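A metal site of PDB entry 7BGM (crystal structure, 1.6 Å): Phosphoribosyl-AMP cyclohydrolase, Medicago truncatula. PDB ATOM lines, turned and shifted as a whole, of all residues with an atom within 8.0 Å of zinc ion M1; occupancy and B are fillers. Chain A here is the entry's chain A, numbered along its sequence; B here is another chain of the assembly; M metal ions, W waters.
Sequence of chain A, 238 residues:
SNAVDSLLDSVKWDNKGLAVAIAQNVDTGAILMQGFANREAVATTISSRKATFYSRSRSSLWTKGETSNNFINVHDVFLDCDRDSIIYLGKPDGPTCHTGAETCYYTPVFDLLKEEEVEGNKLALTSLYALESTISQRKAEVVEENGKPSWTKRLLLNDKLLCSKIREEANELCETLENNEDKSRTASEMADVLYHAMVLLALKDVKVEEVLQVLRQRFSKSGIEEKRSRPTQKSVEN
The backbone NH of Asp 80 sits at hydrogen-bond distance from the backbone carbonyl oxygen of Ser 85 (2.9 Å). The side-chain carboxylate (OD1) of Asp 80 lies within hydrogen-bond range of the backbone NH (N) of Arg 83. The backbone NH of Val 20 sits at hydrogen-bond distance from the backbone carbonyl oxygen of Asp 84, 3.3 Å away.
The nearest printed residue that does not touch zinc ion M1 is Ser 85 (4.2 Å).
Zinc ion M1 is bound by OD2 of Asp 80 (1.9 Å), OD1 of Asp 84 (1.9 Å), OD1 of Asp 82 (2.0 Å), water W1 (2.0 Å) and water W2 (2.1 Å).
Water W1 lies within hydrogen-bond range of OD2 of Asp 82 and OD2 of Asp 84.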
ATOM      1  N   LYS A  12      -6.922 -12.201  25.534  1.00  0.00           N
ATOM      2  CA  LYS A  12      -6.528 -11.532  26.778  1.00  0.00           C
ATOM      3  C   LYS A  12      -7.368 -12.089  27.914  1.00  0.00           C
ATOM      4  O   LYS A  12      -8.364 -11.480  28.354  1.00  0.00           O
ATOM      5  CB  LYS A  12      -6.669 -10.023  26.640  1.00  0.00           C
ATOM      6  CG  LYS A  12      -6.271  -9.195  27.841  1.00  0.00           C
ATOM      7  CD  LYS A  12      -6.593  -7.735  27.541  1.00  0.00           C
ATOM      8  CE  LYS A  12      -6.217  -6.799  28.688  1.00  0.00           C
ATOM      9  NZ  LYS A  12      -6.718  -5.424  28.371  1.00  0.00           N
ATOM     10  N   VAL A  20     -15.098 -12.842  28.585  1.00  0.00           N
ATOM     11  CA  VAL A  20     -16.555 -12.723  28.495  1.00  0.00           C
ATOM     12  C   VAL A  20     -16.987 -13.308  27.164  1.00  0.00           C
ATOM     13  O   VAL A  20     -16.350 -13.035  26.136  1.00  0.00           O
ATOM     14  CB  VAL A  20     -16.992 -11.243  28.594  1.00  0.00           C
ATOM     15  CG1 VAL A  20     -18.472 -11.059  28.189  1.00  0.00           C
ATOM     16  CG2 VAL A  20     -16.752 -10.720  30.004  1.00  0.00           C
ATOM     17  N   LEU A  79     -13.696 -11.685  18.270  1.00  0.00           N
ATOM     18  CA  LEU A  79     -13.067 -11.037  19.414  1.00  0.00           C
ATOM     19  C   LEU A  79     -13.260  -9.525  19.305  1.00  0.00           C
ATOM     20  O   LEU A  79     -13.323  -8.987  18.191  1.00  0.00           O
ATOM     21  CB  LEU A  79     -11.559 -11.323  19.450  1.00  0.00           C
ATOM     22  CG  LEU A  79     -11.105 -12.766  19.586  1.00  0.00           C
ATOM     23  CD1 LEU A  79      -9.574 -12.920  19.489  1.00  0.00           C
ATOM     24  CD2 LEU A  79     -11.596 -13.261  20.914  1.00  0.00           C
ATOM     25  N   ASP A  80     -13.305  -8.836  20.454  1.00  0.00           N
ATOM     26  CA  ASP A  80     -13.306  -7.367  20.444  1.00  0.00           C
ATOM     27  C   ASP A  80     -11.877  -6.826  20.270  1.00  0.00           C
ATOM     28  O   ASP A  80     -10.883  -7.575  20.153  1.00  0.00           O
ATOM     29  CB  ASP A  80     -14.033  -6.756  21.657  1.00  0.00           C
ATOM     30  CG  ASP A  80     -13.234  -6.756  22.958  1.00  0.00           C
ATOM     31  OD1 ASP A  80     -12.384  -7.635  23.109  1.00  0.00           O
ATOM     32  OD2 ASP A  80     -13.580  -5.895  23.848  1.00  0.00           O
ATOM     33  N   CYS A  81     -11.778  -5.505  20.198  1.00  0.00           N
ATOM     34  CA  CYS A  81     -10.518  -4.849  19.814  1.00  0.00           C
ATOM     35  C   CYS A  81      -9.354  -5.208  20.738  1.00  0.00           C
ATOM     36  O   CYS A  81      -8.204  -5.354  20.287  1.00  0.00           O
ATOM     37  CB  CYS A  81     -10.731  -3.339  19.759  1.00  0.00           C
ATOM     38  SG  CYS A  81     -11.345  -2.642  21.384  1.00  0.00           S
ATOM     39  N   ASP A  82      -9.604  -5.331  22.036  1.00  0.00           N
ATOM     40  CA  ASP A  82      -8.534  -5.649  22.982  1.00  0.00           C
ATOM     41  C   ASP A  82      -8.585  -7.123  23.426  1.00  0.00           C
ATOM     42  O   ASP A  82      -7.859  -7.519  24.355  1.00  0.00           O
ATOM     43  CB  ASP A  82      -8.537  -4.683  24.174  1.00  0.00           C
ATOM     44  CG  ASP A  82      -9.879  -4.576  24.895  1.00  0.00           C
ATOM     45  OD1 ASP A  82     -10.792  -5.410  24.661  1.00  0.00           O
ATOM     46  OD2 ASP A  82     -10.014  -3.632  25.738  1.00  0.00           O
ATOM     47  N   ARG A  83      -9.389  -7.942  22.731  1.00  0.00           N
ATOM     48  CA  ARG A  83      -9.342  -9.404  22.734  1.00  0.00           C
ATOM     49  C   ARG A  83      -9.717 -10.010  24.093  1.00  0.00           C
ATOM     50  O   ARG A  83      -9.283 -11.114  24.420  1.00  0.00           O
ATOM     51  CB  ARG A  83      -7.963  -9.904  22.278  1.00  0.00           C
ATOM     52  CG  ARG A  83      -7.458  -9.191  21.036  1.00  0.00           C
ATOM     53  CD  ARG A  83      -6.134  -9.715  20.549  1.00  0.00           C
ATOM     54  NE  ARG A  83      -6.171 -10.985  19.840  1.00  0.00           N
ATOM     55  CZ  ARG A  83      -6.426 -11.115  18.530  1.00  0.00           C
ATOM     56  NH1 ARG A  83      -6.718 -10.055  17.776  1.00  0.00           N
ATOM     57  NH2 ARG A  83      -6.381 -12.300  17.969  1.00  0.00           N
ATOM     58  N   ASP A  84     -10.525  -9.332  24.893  1.00  0.00           N
ATOM     59  CA  ASP A  84     -11.021  -9.935  26.137  1.00  0.00           C
ATOM     60  C   ASP A  84     -12.521 -10.218  26.136  1.00  0.00           C
ATOM     61  O   ASP A  84     -13.084 -10.564  27.187  1.00  0.00           O
ATOM     62  CB  ASP A  84     -10.673  -9.060  27.353  1.00  0.00           C
ATOM     63  CG  ASP A  84     -11.257  -7.647  27.257  1.00  0.00           C
ATOM     64  OD1 ASP A  84     -12.100  -7.390  26.336  1.00  0.00           O
ATOM     65  OD2 ASP A  84     -10.866  -6.811  28.085  1.00  0.00           O
ATOM     66  N   SER A  85     -13.184 -10.086  24.993  1.00  0.00           N
ATOM     67  CA  SER A  85     -14.624 -10.249  24.839  1.00  0.00           C
ATOM     68  C   SER A  85     -14.881 -10.981  23.532  1.00  0.00           C
ATOM     69  O   SER A  85     -14.234 -10.705  22.523  1.00  0.00           O
ATOM     70  CB  SER A  85     -15.289  -8.878  24.832  1.00  0.00           C
ATOM     71  OG  SER A  85     -16.691  -9.029  24.782  1.00  0.00           O
ATOM     72  N   ILE A  86     -15.765 -11.979  23.577  1.00  0.00           N
ATOM     73  CA  ILE A  86     -16.028 -12.881  22.457  1.00  0.00           C
ATOM     74  C   ILE A  86     -17.499 -12.831  22.146  1.00  0.00           C
ATOM     75  O   ILE A  86     -18.312 -12.931  23.066  1.00  0.00           O
ATOM     76  CB  ILE A  86     -15.610 -14.311  22.822  1.00  0.00           C
ATOM     77  CG1 ILE A  86     -14.123 -14.301  23.205  1.00  0.00           C
ATOM     78  CG2 ILE A  86     -15.941 -15.263  21.687  1.00  0.00           C
ATOM     79  CD1 ILE A  86     -13.593 -15.635  23.736  1.00  0.00           C
ATOM     80  N   MET B  33     -19.900  -2.567  22.026  1.00  0.00           N
ATOM     81  CA  MET B  33     -18.768  -2.703  22.942  1.00  0.00           C
ATOM     82  C   MET B  33     -19.255  -3.452  24.172  1.00  0.00           C
ATOM     83  O   MET B  33     -20.462  -3.550  24.432  1.00  0.00           O
ATOM     84  CB  MET B  33     -18.150  -1.355  23.364  1.00  0.00           C
ATOM     85  CG  MET B  33     -19.103  -0.496  24.166  1.00  0.00           C
ATOM     86  SD  MET B  33     -18.291   0.944  24.871  1.00  0.00           S
ATOM     87  CE  MET B  33     -17.396   0.185  26.232  1.00  0.00           C
ATOM     88  N   GLN B  34     -18.293  -3.944  24.963  1.00  0.00           N
ATOM     89  CA  GLN B  34     -18.627  -4.585  26.239  1.00  0.00           C
ATOM     90  C   GLN B  34     -17.586  -4.165  27.261  1.00  0.00           C
ATOM     91  O   GLN B  34     -16.374  -4.181  26.974  1.00  0.00           O
ATOM     92  CB  GLN B  34     -18.679  -6.120  26.126  1.00  0.00           C
ATOM     93  CG  GLN B  34     -18.878  -6.903  27.473  1.00  0.00           C
ATOM     94  CD  GLN B  34     -17.574  -7.442  28.019  1.00  0.00           C
ATOM     95  OE1 GLN B  34     -16.872  -8.206  27.328  1.00  0.00           O
ATOM     96  NE2 GLN B  34     -17.203  -7.043  29.261  1.00  0.00           N
ATOM     97  N   GLY B  35     -18.060  -3.750  28.436  1.00  0.00           N
ATOM     98  CA  GLY B  35     -17.160  -3.447  29.519  1.00  0.00           C
ATOM     99  C   GLY B  35     -17.722  -3.893  30.827  1.00  0.00           C
ATOM    100  O   GLY B  35     -18.456  -4.900  30.869  1.00  0.00           O
ATOM    101  N   PHE B  36     -17.342  -3.221  31.912  1.00  0.00           N
ATOM    102  CA  PHE B  36     -17.838  -3.555  33.230  1.00  0.00           C
ATOM    103  C   PHE B  36     -18.476  -2.323  33.853  1.00  0.00           C
ATOM    104  O   PHE B  36     -18.253  -1.189  33.387  1.00  0.00           O
ATOM    105  CB  PHE B  36     -16.685  -4.120  34.110  1.00  0.00           C
ATOM    106  CG  PHE B  36     -16.232  -5.479  33.645  1.00  0.00           C
ATOM    107  CD1 PHE B  36     -15.328  -5.589  32.598  1.00  0.00           C
ATOM    108  CD2 PHE B  36     -16.778  -6.641  34.185  1.00  0.00           C
ATOM    109  CE1 PHE B  36     -14.928  -6.854  32.126  1.00  0.00           C
ATOM    110  CE2 PHE B  36     -16.383  -7.905  33.729  1.00  0.00           C
ATOM    111  CZ  PHE B  36     -15.450  -8.002  32.677  1.00  0.00           C
ATOM    112  N   ARG B  56     -11.342  -1.547  34.968  1.00  0.00           N
ATOM    113  CA  ARG B  56     -10.600  -2.298  35.979  1.00  0.00           C
ATOM    114  C   ARG B  56      -9.136  -1.868  36.018  1.00  0.00           C
ATOM    115  O   ARG B  56      -8.535  -1.779  37.096  1.00  0.00           O
ATOM    116  CB  ARG B  56     -10.735  -3.805  35.731  1.00  0.00           C
ATOM    117  CG  ARG B  56     -12.188  -4.328  35.838  1.00  0.00           C
ATOM    118  CD  ARG B  56     -12.251  -5.797  35.480  1.00  0.00           C
ATOM    119  NE  ARG B  56     -12.012  -5.959  34.046  1.00  0.00           N
ATOM    120  CZ  ARG B  56     -11.922  -7.135  33.413  1.00  0.00           C
ATOM    121  NH1 ARG B  56     -12.047  -8.274  34.089  1.00  0.00           N
ATOM    122  NH2 ARG B  56     -11.704  -7.152  32.109  1.00  0.00           N
ATOM    123  N   CYS B 104     -16.573  -2.443  18.325  1.00  0.00           N
ATOM    124  CA  CYS B 104     -15.342  -3.095  18.776  1.00  0.00           C
ATOM    125  C   CYS B 104     -15.147  -4.493  18.211  1.00  0.00           C
ATOM    126  O   CYS B 104     -14.081  -5.070  18.461  1.00  0.00           O
ATOM    127  CB  CYS B 104     -15.280  -3.182  20.312  1.00  0.00           C
ATOM    128  SG  CYS B 104     -15.192  -1.557  21.121  1.00  0.00           S
ATOM    129  N   TYR B 105     -16.093  -5.053  17.423  1.00  0.00           N
ATOM    130  CA  TYR B 105     -16.038  -6.483  17.063  1.00  0.00           C
ATOM    131  C   TYR B 105     -15.817  -6.629  15.570  1.00  0.00           C
ATOM    132  O   TYR B 105     -16.763  -6.587  14.779  1.00  0.00           O
ATOM    133  CB  TYR B 105     -17.323  -7.230  17.530  1.00  0.00           C
ATOM    134  CG  TYR B 105     -17.468  -7.233  19.032  1.00  0.00           C
ATOM    135  CD1 TYR B 105     -18.108  -6.188  19.688  1.00  0.00           C
ATOM    136  CD2 TYR B 105     -16.976  -8.320  19.779  1.00  0.00           C
ATOM    137  CE1 TYR B 105     -18.219  -6.201  21.122  1.00  0.00           C
ATOM    138  CE2 TYR B 105     -17.115  -8.351  21.189  1.00  0.00           C
ATOM    139  CZ  TYR B 105     -17.742  -7.281  21.829  1.00  0.00           C
ATOM    140  OH  TYR B 105     -17.899  -7.267  23.190  1.00  0.00           O
HETATM  141 ZN    ZN M   1     -12.596  -5.755  25.468  1.00  0.00          ZN
HETATM  142 ZN    ZN M   2      -8.992  -1.697  21.965  1.00  0.00          ZN
HETATM  143 ZN    ZN M   3     -12.956  -1.137  20.759  1.00  0.00          ZN
HETATM  144  O   HOH W   1     -12.345  -4.072  26.560  1.00  0.00           O
HETATM  145  O   HOH W   2     -14.377  -5.918  26.618  1.00  0.00           O
